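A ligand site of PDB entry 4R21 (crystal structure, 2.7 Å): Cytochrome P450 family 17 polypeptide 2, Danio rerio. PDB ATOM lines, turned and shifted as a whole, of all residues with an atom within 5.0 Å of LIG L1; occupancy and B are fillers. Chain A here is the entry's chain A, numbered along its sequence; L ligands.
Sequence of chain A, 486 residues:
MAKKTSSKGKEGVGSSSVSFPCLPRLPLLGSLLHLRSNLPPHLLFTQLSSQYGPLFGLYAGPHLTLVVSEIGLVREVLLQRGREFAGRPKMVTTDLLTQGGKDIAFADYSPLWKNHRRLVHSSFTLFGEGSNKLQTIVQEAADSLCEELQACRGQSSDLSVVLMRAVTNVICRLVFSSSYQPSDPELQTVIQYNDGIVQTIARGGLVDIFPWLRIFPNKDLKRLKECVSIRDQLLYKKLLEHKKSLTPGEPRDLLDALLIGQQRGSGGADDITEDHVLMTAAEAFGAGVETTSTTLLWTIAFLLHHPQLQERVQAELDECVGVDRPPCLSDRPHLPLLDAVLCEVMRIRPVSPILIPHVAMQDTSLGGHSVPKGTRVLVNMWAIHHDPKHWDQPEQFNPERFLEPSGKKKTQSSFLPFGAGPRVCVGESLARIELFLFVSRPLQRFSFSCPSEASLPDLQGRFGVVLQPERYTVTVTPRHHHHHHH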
ATOM      1  N   LEU A  78     -18.281 -39.209 -17.131  1.00  0.00           N
ATOM      2  CA  LEU A  78     -18.429 -38.450 -18.342  1.00  0.00           C
ATOM      3  C   LEU A  78     -18.175 -39.284 -19.579  1.00  0.00           C
ATOM      4  O   LEU A  78     -19.012 -39.336 -20.479  1.00  0.00           O
ATOM      5  CB  LEU A  78     -17.521 -37.223 -18.318  1.00  0.00           C
ATOM      6  CG  LEU A  78     -17.773 -36.150 -17.262  1.00  0.00           C
ATOM      7  CD1 LEU A  78     -16.778 -35.021 -17.434  1.00  0.00           C
ATOM      8  CD2 LEU A  78     -19.202 -35.589 -17.289  1.00  0.00           C
ATOM      9  N   ARG A  88     -30.724 -35.448 -17.185  1.00  0.00           N
ATOM     10  CA  ARG A  88     -30.786 -34.133 -16.502  1.00  0.00           C
ATOM     11  C   ARG A  88     -31.998 -34.033 -15.595  1.00  0.00           C
ATOM     12  O   ARG A  88     -32.993 -34.745 -15.743  1.00  0.00           O
ATOM     13  CB  ARG A  88     -30.782 -32.977 -17.497  1.00  0.00           C
ATOM     14  CG  ARG A  88     -29.540 -32.879 -18.348  1.00  0.00           C
ATOM     15  CD  ARG A  88     -28.287 -32.604 -17.543  1.00  0.00           C
ATOM     16  NE  ARG A  88     -27.282 -31.950 -18.374  1.00  0.00           N
ATOM     17  CZ  ARG A  88     -25.992 -31.805 -18.063  1.00  0.00           C
ATOM     18  NH1 ARG A  88     -25.467 -32.271 -16.932  1.00  0.00           N
ATOM     19  NH2 ARG A  88     -25.225 -31.151 -18.909  1.00  0.00           N
ATOM     20  N   ILE A 104     -30.984 -27.928 -25.047  1.00  0.00           N
ATOM     21  CA  ILE A 104     -29.968 -28.990 -24.932  1.00  0.00           C
ATOM     22  C   ILE A 104     -29.486 -29.290 -23.495  1.00  0.00           C
ATOM     23  O   ILE A 104     -29.362 -30.456 -23.092  1.00  0.00           O
ATOM     24  CB  ILE A 104     -28.728 -28.609 -25.760  1.00  0.00           C
ATOM     25  CG1 ILE A 104     -29.088 -28.535 -27.243  1.00  0.00           C
ATOM     26  CG2 ILE A 104     -27.575 -29.602 -25.496  1.00  0.00           C
ATOM     27  CD1 ILE A 104     -29.577 -29.852 -27.819  1.00  0.00           C
ATOM     28  N   ALA A 105     -29.199 -28.244 -22.743  1.00  0.00           N
ATOM     29  CA  ALA A 105     -28.515 -28.403 -21.446  1.00  0.00           C
ATOM     30  C   ALA A 105     -29.360 -29.141 -20.393  1.00  0.00           C
ATOM     31  O   ALA A 105     -28.866 -30.032 -19.717  1.00  0.00           O
ATOM     32  CB  ALA A 105     -28.029 -27.043 -20.920  1.00  0.00           C
ATOM     33  N   TRP A 113     -33.106 -36.043 -28.454  1.00  0.00           N
ATOM     34  CA  TRP A 113     -32.024 -35.177 -28.007  1.00  0.00           C
ATOM     35  C   TRP A 113     -30.730 -35.434 -28.811  1.00  0.00           C
ATOM     36  O   TRP A 113     -29.940 -34.515 -29.033  1.00  0.00           O
ATOM     37  CB  TRP A 113     -31.824 -35.319 -26.484  1.00  0.00           C
ATOM     38  CG  TRP A 113     -30.735 -34.493 -25.934  1.00  0.00           C
ATOM     39  CD1 TRP A 113     -30.849 -33.275 -25.363  1.00  0.00           C
ATOM     40  CD2 TRP A 113     -29.352 -34.827 -25.894  1.00  0.00           C
ATOM     41  NE1 TRP A 113     -29.610 -32.830 -24.948  1.00  0.00           N
ATOM     42  CE2 TRP A 113     -28.671 -33.765 -25.278  1.00  0.00           C
ATOM     43  CE3 TRP A 113     -28.616 -35.948 -26.314  1.00  0.00           C
ATOM     44  CZ2 TRP A 113     -27.294 -33.770 -25.116  1.00  0.00           C
ATOM     45  CZ3 TRP A 113     -27.262 -35.956 -26.113  1.00  0.00           C
ATOM     46  CH2 TRP A 113     -26.608 -34.879 -25.537  1.00  0.00           C
ATOM     47  N   PHE A 124     -22.819 -25.314 -35.691  1.00  0.00           N
ATOM     48  CA  PHE A 124     -21.683 -24.530 -35.183  1.00  0.00           C
ATOM     49  C   PHE A 124     -20.430 -24.790 -35.990  1.00  0.00           C
ATOM     50  O   PHE A 124     -19.708 -23.845 -36.328  1.00  0.00           O
ATOM     51  CB  PHE A 124     -21.388 -24.844 -33.722  1.00  0.00           C
ATOM     52  CG  PHE A 124     -22.359 -24.229 -32.750  1.00  0.00           C
ATOM     53  CD1 PHE A 124     -22.474 -22.854 -32.651  1.00  0.00           C
ATOM     54  CD2 PHE A 124     -23.141 -25.015 -31.939  1.00  0.00           C
ATOM     55  CE1 PHE A 124     -23.359 -22.275 -31.755  1.00  0.00           C
ATOM     56  CE2 PHE A 124     -24.035 -24.440 -31.055  1.00  0.00           C
ATOM     57  CZ  PHE A 124     -24.153 -23.073 -30.958  1.00  0.00           C
ATOM     58  N   GLU A 283     -30.768 -20.545 -25.786  1.00  0.00           N
ATOM     59  CA  GLU A 283     -29.646 -21.139 -25.074  1.00  0.00           C
ATOM     60  C   GLU A 283     -28.274 -20.670 -25.578  1.00  0.00           C
ATOM     61  O   GLU A 283     -27.327 -20.657 -24.809  1.00  0.00           O
ATOM     62  CB  GLU A 283     -29.715 -22.648 -25.147  1.00  0.00           C
ATOM     63  CG  GLU A 283     -28.760 -23.319 -24.196  1.00  0.00           C
ATOM     64  CD  GLU A 283     -29.345 -24.581 -23.637  1.00  0.00           C
ATOM     65  OE1 GLU A 283     -29.095 -25.670 -24.195  1.00  0.00           O
ATOM     66  OE2 GLU A 283     -30.091 -24.473 -22.648  1.00  0.00           O
ATOM     67  N   ALA A 284     -28.157 -20.314 -26.849  1.00  0.00           N
ATOM     68  CA  ALA A 284     -26.860 -19.858 -27.315  1.00  0.00           C
ATOM     69  C   ALA A 284     -26.403 -18.654 -26.512  1.00  0.00           C
ATOM     70  O   ALA A 284     -25.220 -18.461 -26.292  1.00  0.00           O
ATOM     71  CB  ALA A 284     -26.874 -19.581 -28.811  1.00  0.00           C
ATOM     72  N   ALA A 287     -26.167 -20.126 -22.303  1.00  0.00           N
ATOM     73  CA  ALA A 287     -24.922 -20.828 -22.095  1.00  0.00           C
ATOM     74  C   ALA A 287     -23.702 -20.083 -22.557  1.00  0.00           C
ATOM     75  O   ALA A 287     -22.586 -20.321 -22.052  1.00  0.00           O
ATOM     76  CB  ALA A 287     -24.972 -22.156 -22.824  1.00  0.00           C
ATOM     77  N   GLY A 288     -23.854 -19.214 -23.548  1.00  0.00           N
ATOM     78  CA  GLY A 288     -22.697 -18.649 -24.234  1.00  0.00           C
ATOM     79  C   GLY A 288     -22.163 -17.331 -23.751  1.00  0.00           C
ATOM     80  O   GLY A 288     -20.989 -17.037 -23.928  1.00  0.00           O
ATOM     81  N   THR A 291     -20.548 -17.242 -19.669  1.00  0.00           N
ATOM     82  CA  THR A 291     -19.334 -18.055 -19.660  1.00  0.00           C
ATOM     83  C   THR A 291     -18.200 -17.382 -20.423  1.00  0.00           C
ATOM     84  O   THR A 291     -17.031 -17.391 -19.978  1.00  0.00           O
ATOM     85  CB  THR A 291     -19.577 -19.412 -20.318  1.00  0.00           C
ATOM     86  OG1 THR A 291     -20.165 -19.223 -21.629  1.00  0.00           O
ATOM     87  CG2 THR A 291     -20.475 -20.297 -19.434  1.00  0.00           C
ATOM     88  N   THR A 292     -18.524 -16.833 -21.595  1.00  0.00           N
ATOM     89  CA  THR A 292     -17.480 -16.258 -22.420  1.00  0.00           C
ATOM     90  C   THR A 292     -17.042 -14.947 -21.790  1.00  0.00           C
ATOM     91  O   THR A 292     -15.851 -14.797 -21.496  1.00  0.00           O
ATOM     92  CB  THR A 292     -17.923 -16.055 -23.862  1.00  0.00           C
ATOM     93  OG1 THR A 292     -19.261 -15.511 -23.862  1.00  0.00           O
ATOM     94  CG2 THR A 292     -17.954 -17.345 -24.592  1.00  0.00           C
ATOM     95  N   THR A 295     -14.844 -15.566 -18.757  1.00  0.00           N
ATOM     96  CA  THR A 295     -13.542 -16.086 -19.067  1.00  0.00           C
ATOM     97  C   THR A 295     -12.617 -14.948 -19.525  1.00  0.00           C
ATOM     98  O   THR A 295     -11.444 -14.922 -19.152  1.00  0.00           O
ATOM     99  CB  THR A 295     -13.612 -17.188 -20.107  1.00  0.00           C
ATOM    100  OG1 THR A 295     -14.558 -18.193 -19.698  1.00  0.00           O
ATOM    101  CG2 THR A 295     -12.288 -17.821 -20.290  1.00  0.00           C
ATOM    102  N   MET A 346      -8.810 -20.890 -17.819  1.00  0.00           N
ATOM    103  CA  MET A 346      -9.921 -21.821 -17.757  1.00  0.00           C
ATOM    104  C   MET A 346      -9.740 -22.875 -16.675  1.00  0.00           C
ATOM    105  O   MET A 346     -10.725 -23.338 -16.109  1.00  0.00           O
ATOM    106  CB  MET A 346     -10.142 -22.500 -19.100  1.00  0.00           C
ATOM    107  CG  MET A 346     -10.825 -21.662 -20.189  1.00  0.00           C
ATOM    108  SD  MET A 346     -10.712 -22.706 -21.663  1.00  0.00           S
ATOM    109  CE  MET A 346     -11.849 -21.966 -22.793  1.00  0.00           C
ATOM    110  N   VAL A 351     -15.391 -21.525 -14.740  1.00  0.00           N
ATOM    111  CA  VAL A 351     -16.693 -20.826 -14.769  1.00  0.00           C
ATOM    112  C   VAL A 351     -17.856 -21.565 -14.044  1.00  0.00           C
ATOM    113  O   VAL A 351     -18.694 -20.925 -13.444  1.00  0.00           O
ATOM    114  CB  VAL A 351     -17.136 -20.469 -16.220  1.00  0.00           C
ATOM    115  CG1 VAL A 351     -16.314 -19.307 -16.772  1.00  0.00           C
ATOM    116  CG2 VAL A 351     -17.043 -21.650 -17.155  1.00  0.00           C
ATOM    117  N   LEU A 355     -20.542 -28.775 -12.162  1.00  0.00           N
ATOM    118  CA  LEU A 355     -21.380 -28.839 -13.350  1.00  0.00           C
ATOM    119  C   LEU A 355     -22.869 -28.968 -12.996  1.00  0.00           C
ATOM    120  O   LEU A 355     -23.216 -29.227 -11.858  1.00  0.00           O
ATOM    121  CB  LEU A 355     -20.949 -29.983 -14.280  1.00  0.00           C
ATOM    122  CG  LEU A 355     -19.488 -29.984 -14.687  1.00  0.00           C
ATOM    123  CD1 LEU A 355     -19.181 -31.142 -15.644  1.00  0.00           C
ATOM    124  CD2 LEU A 355     -19.115 -28.632 -15.286  1.00  0.00           C
ATOM    125  N   ILE A 356     -23.725 -28.806 -14.014  1.00  0.00           N
ATOM    126  CA  ILE A 356     -25.157 -29.058 -13.908  1.00  0.00           C
ATOM    127  C   ILE A 356     -25.170 -30.531 -13.538  1.00  0.00           C
ATOM    128  O   ILE A 356     -24.310 -31.274 -13.977  1.00  0.00           O
ATOM    129  CB  ILE A 356     -25.908 -28.843 -15.276  1.00  0.00           C
ATOM    130  CG1 ILE A 356     -25.680 -27.474 -15.923  1.00  0.00           C
ATOM    131  CG2 ILE A 356     -27.415 -29.024 -15.171  1.00  0.00           C
ATOM    132  CD1 ILE A 356     -25.785 -27.552 -17.444  1.00  0.00           C
ATOM    133  N   HIS A 358     -25.399 -34.464 -13.471  1.00  0.00           N
ATOM    134  CA  HIS A 358     -25.594 -35.575 -14.388  1.00  0.00           C
ATOM    135  C   HIS A 358     -26.454 -36.597 -13.721  1.00  0.00           C
ATOM    136  O   HIS A 358     -26.042 -37.132 -12.673  1.00  0.00           O
ATOM    137  CB  HIS A 358     -24.280 -36.247 -14.709  1.00  0.00           C
ATOM    138  CG  HIS A 358     -23.525 -35.588 -15.812  1.00  0.00           C
ATOM    139  ND1 HIS A 358     -22.959 -34.340 -15.660  1.00  0.00           N
ATOM    140  CD2 HIS A 358     -23.233 -35.980 -17.068  1.00  0.00           C
ATOM    141  CE1 HIS A 358     -22.357 -33.985 -16.785  1.00  0.00           C
ATOM    142  NE2 HIS A 358     -22.512 -34.972 -17.646  1.00  0.00           N
ATOM    143  N   MET A 381     -15.486 -29.583 -10.732  1.00  0.00           N
ATOM    144  CA  MET A 381     -14.537 -29.157 -11.729  1.00  0.00           C
ATOM    145  C   MET A 381     -13.351 -28.459 -11.079  1.00  0.00           C
ATOM    146  O   MET A 381     -12.237 -28.498 -11.606  1.00  0.00           O
ATOM    147  CB  MET A 381     -15.238 -28.257 -12.740  1.00  0.00           C
ATOM    148  CG  MET A 381     -14.495 -28.208 -14.067  1.00  0.00           C
ATOM    149  SD  MET A 381     -15.312 -29.032 -15.462  1.00  0.00           S
ATOM    150  CE  MET A 381     -15.157 -30.736 -14.956  1.00  0.00           C
ATOM    151  N   PRO A 417     -11.951 -28.539 -19.388  1.00  0.00           N
ATOM    152  CA  PRO A 417     -12.667 -27.258 -19.344  1.00  0.00           C
ATOM    153  C   PRO A 417     -14.040 -27.286 -19.970  1.00  0.00           C
ATOM    154  O   PRO A 417     -14.928 -26.533 -19.521  1.00  0.00           O
ATOM    155  CB  PRO A 417     -11.765 -26.295 -20.127  1.00  0.00           C
ATOM    156  CG  PRO A 417     -10.928 -27.185 -20.967  1.00  0.00           C
ATOM    157  CD  PRO A 417     -10.684 -28.412 -20.129  1.00  0.00           C
ATOM    158  N   PHE A 418     -14.239 -28.155 -20.942  1.00  0.00           N
ATOM    159  CA  PHE A 418     -15.532 -28.264 -21.575  1.00  0.00           C
ATOM    160  C   PHE A 418     -16.348 -29.510 -21.213  1.00  0.00           C
ATOM    161  O   PHE A 418     -17.250 -29.890 -21.924  1.00  0.00           O
ATOM    162  CB  PHE A 418     -15.327 -28.146 -23.105  1.00  0.00           C
ATOM    163  CG  PHE A 418     -14.807 -26.807 -23.535  1.00  0.00           C
ATOM    164  CD1 PHE A 418     -15.671 -25.733 -23.721  1.00  0.00           C
ATOM    165  CD2 PHE A 418     -13.445 -26.591 -23.675  1.00  0.00           C
ATOM    166  CE1 PHE A 418     -15.195 -24.492 -24.081  1.00  0.00           C
ATOM    167  CE2 PHE A 418     -12.958 -25.354 -24.070  1.00  0.00           C
ATOM    168  CZ  PHE A 418     -13.831 -24.302 -24.280  1.00  0.00           C
ATOM    169  N   GLY A 419     -16.073 -30.155 -20.100  1.00  0.00           N
ATOM    170  CA  GLY A 419     -16.608 -31.506 -19.909  1.00  0.00           C
ATOM    171  C   GLY A 419     -16.075 -32.508 -20.944  1.00  0.00           C
ATOM    172  O   GLY A 419     -14.941 -32.411 -21.396  1.00  0.00           O
ATOM    173  N   ARG A 423     -22.287 -35.450 -23.001  1.00  0.00           N
ATOM    174  CA  ARG A 423     -22.802 -34.146 -22.571  1.00  0.00           C
ATOM    175  C   ARG A 423     -21.809 -33.009 -22.697  1.00  0.00           C
ATOM    176  O   ARG A 423     -22.020 -31.961 -22.109  1.00  0.00           O
ATOM    177  CB  ARG A 423     -23.238 -34.257 -21.083  1.00  0.00           C
ATOM    178  CG  ARG A 423     -24.577 -34.958 -20.881  1.00  0.00           C
ATOM    179  CD  ARG A 423     -25.621 -34.030 -21.493  1.00  0.00           C
ATOM    180  NE  ARG A 423     -26.931 -34.599 -21.731  1.00  0.00           N
ATOM    181  CZ  ARG A 423     -28.023 -33.868 -21.893  1.00  0.00           C
ATOM    182  NH1 ARG A 423     -27.971 -32.527 -21.850  1.00  0.00           N
ATOM    183  NH2 ARG A 423     -29.175 -34.483 -22.110  1.00  0.00           N
ATOM    184  N   VAL A 424     -20.702 -33.257 -23.381  1.00  0.00           N
ATOM    185  CA  VAL A 424     -19.657 -32.233 -23.678  1.00  0.00           C
ATOM    186  C   VAL A 424     -20.174 -30.930 -24.275  1.00  0.00           C
ATOM    187  O   VAL A 424     -21.180 -30.903 -24.982  1.00  0.00           O
ATOM    188  CB  VAL A 424     -18.610 -32.816 -24.675  1.00  0.00           C
ATOM    189  CG1 VAL A 424     -19.254 -33.178 -25.998  1.00  0.00           C
ATOM    190  CG2 VAL A 424     -17.436 -31.862 -24.881  1.00  0.00           C
ATOM    191  N   CYS A 425     -19.462 -29.840 -24.034  1.00  0.00           N
ATOM    192  CA  CYS A 425     -19.935 -28.559 -24.498  1.00  0.00           C
ATOM    193  C   CYS A 425     -20.240 -28.599 -25.994  1.00  0.00           C
ATOM    194  O   CYS A 425     -19.411 -29.040 -26.780  1.00  0.00           O
ATOM    195  CB  CYS A 425     -18.905 -27.494 -24.212  1.00  0.00           C
ATOM    196  SG  CYS A 425     -19.521 -25.834 -24.546  1.00  0.00           S
ATOM    197  N   VAL A 426     -21.432 -28.183 -26.377  1.00  0.00           N
ATOM    198  CA  VAL A 426     -21.762 -28.070 -27.813  1.00  0.00           C
ATOM    199  C   VAL A 426     -21.238 -26.794 -28.459  1.00  0.00           C
ATOM    200  O   VAL A 426     -21.247 -26.715 -29.670  1.00  0.00           O
ATOM    201  CB  VAL A 426     -23.271 -28.177 -28.140  1.00  0.00           C
ATOM    202  CG1 VAL A 426     -23.766 -29.553 -27.803  1.00  0.00           C
ATOM    203  CG2 VAL A 426     -24.073 -27.155 -27.357  1.00  0.00           C
ATOM    204  N   GLY A 427     -20.780 -25.822 -27.659  1.00  0.00           N
ATOM    205  CA  GLY A 427     -20.252 -24.546 -28.146  1.00  0.00           C
ATOM    206  C   GLY A 427     -18.773 -24.357 -27.882  1.00  0.00           C
ATOM    207  O   GLY A 427     -18.300 -23.218 -27.757  1.00  0.00           O
ATOM    208  N   LEU A 430     -16.915 -22.924 -30.825  1.00  0.00           N
ATOM    209  CA  LEU A 430     -17.268 -21.537 -30.933  1.00  0.00           C
ATOM    210  C   LEU A 430     -16.608 -20.720 -29.834  1.00  0.00           C
ATOM    211  O   LEU A 430     -16.147 -19.600 -30.062  1.00  0.00           O
ATOM    212  CB  LEU A 430     -18.765 -21.414 -30.880  1.00  0.00           C
ATOM    213  CG  LEU A 430     -19.191 -20.006 -31.145  1.00  0.00           C
ATOM    214  CD1 LEU A 430     -20.529 -20.075 -31.832  1.00  0.00           C
ATOM    215  CD2 LEU A 430     -19.303 -19.210 -29.858  1.00  0.00           C
ATOM    216  N   ALA A 431     -16.606 -21.266 -28.639  1.00  0.00           N
ATOM    217  CA  ALA A 431     -16.021 -20.610 -27.478  1.00  0.00           C
ATOM    218  C   ALA A 431     -14.546 -20.304 -27.695  1.00  0.00           C
ATOM    219  O   ALA A 431     -14.096 -19.168 -27.532  1.00  0.00           O
ATOM    220  CB  ALA A 431     -16.163 -21.527 -26.259  1.00  0.00           C
ATOM    221  N   GLU A 434     -14.053 -17.732 -30.293  1.00  0.00           N
ATOM    222  CA  GLU A 434     -14.376 -16.468 -29.644  1.00  0.00           C
ATOM    223  C   GLU A 434     -13.172 -15.978 -28.792  1.00  0.00           C
ATOM    224  O   GLU A 434     -12.648 -14.903 -29.007  1.00  0.00           O
ATOM    225  CB  GLU A 434     -15.646 -16.620 -28.798  1.00  0.00           C
ATOM    226  CG  GLU A 434     -16.753 -15.597 -29.044  1.00  0.00           C
ATOM    227  CD  GLU A 434     -18.050 -15.837 -28.210  1.00  0.00           C
ATOM    228  OE1 GLU A 434     -18.294 -16.975 -27.699  1.00  0.00           O
ATOM    229  OE2 GLU A 434     -18.851 -14.880 -28.057  1.00  0.00           O
ATOM    230  N   LEU A 435     -12.704 -16.804 -27.845  1.00  0.00           N
ATOM    231  CA  LEU A 435     -11.699 -16.298 -26.876  1.00  0.00           C
ATOM    232  C   LEU A 435     -10.353 -16.061 -27.540  1.00  0.00           C
ATOM    233  O   LEU A 435      -9.631 -15.137 -27.171  1.00  0.00           O
ATOM    234  CB  LEU A 435     -11.479 -17.258 -25.717  1.00  0.00           C
ATOM    235  CG  LEU A 435     -12.678 -17.606 -24.840  1.00  0.00           C
ATOM    236  CD1 LEU A 435     -12.381 -18.923 -24.145  1.00  0.00           C
ATOM    237  CD2 LEU A 435     -12.948 -16.506 -23.835  1.00  0.00           C
HETATM  238  C1  LIG L   1     -22.077 -27.365 -21.550  1.00  0.00           C
HETATM  239  C2  LIG L   1     -17.897 -25.193 -20.622  1.00  0.00           C
HETATM  240  C3  LIG L   1     -19.076 -21.668 -23.700  1.00  0.00           C
HETATM  241  C4  LIG L   1     -22.994 -24.100 -25.021  1.00  0.00           C
HETATM  242  C5  LIG L   1     -20.842 -27.073 -21.030  1.00  0.00           C
HETATM  243  C6  LIG L   1     -20.256 -27.697 -19.892  1.00  0.00           C
HETATM  244  C7  LIG L   1     -19.076 -27.054 -19.661  1.00  0.00           C
HETATM  245  C8  LIG L   1     -18.936 -26.069 -20.647  1.00  0.00           C
HETATM  246  C9  LIG L   1     -18.047 -27.336 -18.598  1.00  0.00           C
HETATM  247  C10 LIG L   1     -20.808 -28.802 -19.039  1.00  0.00           C
HETATM  248  C11 LIG L   1     -21.106 -30.101 -19.720  1.00  0.00           C
HETATM  249  C12 LIG L   1     -21.585 -30.985 -18.609  1.00  0.00           C
HETATM  250  O1  LIG L   1     -20.947 -31.985 -18.237  1.00  0.00           O
HETATM  251  O2  LIG L   1     -22.634 -30.686 -18.047  1.00  0.00           O
HETATM  252  C13 LIG L   1     -17.918 -24.017 -21.348  1.00  0.00           C
HETATM  253  C14 LIG L   1     -16.900 -23.040 -21.191  1.00  0.00           C
HETATM  254  C15 LIG L   1     -17.201 -22.035 -22.045  1.00  0.00           C
HETATM  255  C16 LIG L   1     -18.453 -22.416 -22.718  1.00  0.00           C
HETATM  256  C17 LIG L   1     -15.698 -23.055 -20.289  1.00  0.00           C
HETATM  257  C18 LIG L   1     -16.338 -20.843 -22.123  1.00  0.00           C
HETATM  258  C19 LIG L   1     -16.651 -19.729 -22.751  1.00  0.00           C
HETATM  259  C20 LIG L   1     -20.231 -22.033 -24.382  1.00  0.00           C
HETATM  260  C21 LIG L   1     -20.804 -21.321 -25.458  1.00  0.00           C
HETATM  261  C22 LIG L   1     -21.941 -22.011 -25.839  1.00  0.00           C
HETATM  262  C23 LIG L   1     -22.039 -23.158 -25.008  1.00  0.00           C
HETATM  263  C24 LIG L   1     -20.313 -20.030 -26.101  1.00  0.00           C
HETATM  264  C25 LIG L   1     -22.781 -21.512 -26.944  1.00  0.00           C
HETATM  265  C26 LIG L   1     -23.921 -22.038 -27.391  1.00  0.00           C
HETATM  266  C27 LIG L   1     -23.000 -25.156 -24.108  1.00  0.00           C
HETATM  267  C28 LIG L   1     -24.146 -26.052 -24.068  1.00  0.00           C
HETATM  268  C29 LIG L   1     -23.926 -26.943 -23.133  1.00  0.00           C
HETATM  269  C30 LIG L   1     -22.621 -26.595 -22.567  1.00  0.00           C
HETATM  270  C31 LIG L   1     -25.395 -26.017 -24.902  1.00  0.00           C
HETATM  271  C32 LIG L   1     -24.880 -28.036 -22.762  1.00  0.00           C
HETATM  272  C33 LIG L   1     -24.420 -29.458 -23.114  1.00  0.00           C
HETATM  273  C34 LIG L   1     -25.284 -30.403 -22.303  1.00  0.00           C
HETATM  274  O3  LIG L   1     -25.560 -31.492 -22.822  1.00  0.00           O
HETATM  275  N1  LIG L   1     -20.025 -26.044 -21.466  1.00  0.00           N
HETATM  276  N2  LIG L   1     -18.767 -23.647 -22.277  1.00  0.00           N
HETATM  277  N3  LIG L   1     -20.986 -23.147 -24.145  1.00  0.00           N
HETATM  278  N4  LIG L   1     -22.087 -25.553 -23.222  1.00  0.00           N
HETATM  279 FE1  LIG L   1     -20.507 -24.671 -22.787  1.00  0.00          FE
HETATM  280  C1  LG2 L   2     -26.767 -18.896 -17.357  1.00  0.00           C
HETATM  281  C2  LG2 L   2     -27.745 -17.756 -17.580  1.00  0.00           C
HETATM  282  C3  LG2 L   2     -28.751 -18.052 -18.454  1.00  0.00           C
HETATM  283  O1  LG2 L   2     -29.358 -17.131 -19.001  1.00  0.00           O
HETATM  284  C4  LG2 L   2     -29.124 -19.366 -18.738  1.00  0.00           C
HETATM  285  C5  LG2 L   2     -28.456 -20.470 -18.211  1.00  0.00           C
HETATM  286  C6  LG2 L   2     -28.900 -21.755 -18.581  1.00  0.00           C
HETATM  287  C7  LG2 L   2     -27.802 -22.570 -19.224  1.00  0.00           C
HETATM  288  C8  LG2 L   2     -26.636 -22.644 -18.271  1.00  0.00           C
HETATM  289  C9  LG2 L   2     -26.201 -21.250 -17.840  1.00  0.00           C
HETATM  290  C10 LG2 L   2     -27.360 -20.351 -17.319  1.00  0.00           C
HETATM  291  C11 LG2 L   2     -24.999 -21.331 -16.819  1.00  0.00           C
HETATM  292  C12 LG2 L   2     -23.839 -22.062 -17.486  1.00  0.00           C
HETATM  293  C13 LG2 L   2     -24.282 -23.454 -17.911  1.00  0.00           C
HETATM  294  C14 LG2 L   2     -25.374 -23.243 -18.955  1.00  0.00           C
HETATM  295  C15 LG2 L   2     -25.509 -24.607 -19.602  1.00  0.00           C
HETATM  296  C16 LG2 L   2     -24.062 -25.192 -19.562  1.00  0.00           C
HETATM  297  C17 LG2 L   2     -23.205 -24.226 -18.714  1.00  0.00           C
HETATM  298  C18 LG2 L   2     -24.734 -24.254 -16.683  1.00  0.00           C
HETATM  299  C19 LG2 L   2     -27.775 -20.731 -15.883  1.00  0.00           C
HETATM  300  C20 LG2 L   2     -22.085 -24.923 -17.840  1.00  0.00           C
HETATM  301  O2  LG2 L   2     -20.954 -24.418 -17.775  1.00  0.00           O
HETATM  302  C21 LG2 L   2     -22.372 -26.222 -17.019  1.00  0.00           C
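An iron atom (FE1) of LIG L1 is bound by the side-chain sulfur (SG) of Cys 425 (2.3 Å).
The guanidinium group of Arg 423 lies within hydrogen-bond range of an oxygen (O3) of LIG L1 (2.8 Å).
A ring nitrogen (NE2) of His 358 lies close to an oxygen (O1) of LIG L1, at 3.4 Å.
An oxygen (O2) of LIG L1 lies within salt-bridge range of the guanidinium group of Arg 88 (2.8 Å).
Merely in contact with LIG L1: Ile 104 (3.8 Å), Ala 105 (3.8 Å), Trp 113 (3.7 Å), Phe 124 (3.7 Å), Glu 283 (3.8 Å), Ala 284 (3.7 Å), Ala 287 (3.5 Å), Gly 288 (3.3 Å), Thr 291 (3.4 Å), Thr 292 (3.3 Å), Val 351 (3.7 Å), Leu 355 (3.2 Å), Pro 417 (3.4 Å), Phe 418 (3.7 Å), Gly 419 (3.8 Å), Val 426 (3.0 Å), Gly 427 (3.8 Å), Leu 430 (3.98 Å), Ala 431 (3.9 Å) and Glu 434 (3.995 Å).
Hydrophobic or aromatic side chains that line LIG L1: Ile 104, Ala 105, Trp 113, Phe 124, Ala 287, Val 351, Leu 355, His 358, Phe 418, Val 426, Leu 430 and Ala 431.
Within 4 Å of LIG L1: Arg 88, Ile 104, Ala 105, Trp 113, Phe 124, Glu 283, Ala 284, Ala 287, Gly 288, Thr 291, Thr 292, Val 351, Leu 355, His 358, Pro 417, Phe 418, Gly 419, Arg 423, Cys 425, Val 426, Gly 427, Leu 430, Ala 431 and Glu 434.
The nearest printed residue that does not touch LIG L1 is Thr 295 (4.01 Å).
OG1 of Thr 291 is in hydrogen-bond range of O of Gly 288 (3.3 Å).
OG1 of Thr 295 lies within hydrogen-bond range of O of Thr 291, at 2.6 Å.
NE1 of Trp 113 is in hydrogen-bond range of O of Ile 104, 3.0 Å away.
The side-chain carboxylate (OE1) of Glu 283 sits at hydrogen-bond distance from the backbone NH (N) of Ala 105, 3.0 Å away.
The backbone NH of Ile 104 lies within hydrogen-bond range of the side-chain carboxylate of Glu 283.
The backbone carbonyl oxygen (O) of Ile 104 sits at hydrogen-bond distance from the guanidinium group (NH1) of Arg 423.
N of Cys 425 is in hydrogen-bond range of O of Phe 418 (3.1 Å).
The guanidinium group of Arg 423 is in hydrogen-bond range of the backbone carbonyl oxygen of Ala 105, at 3.4 Å.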
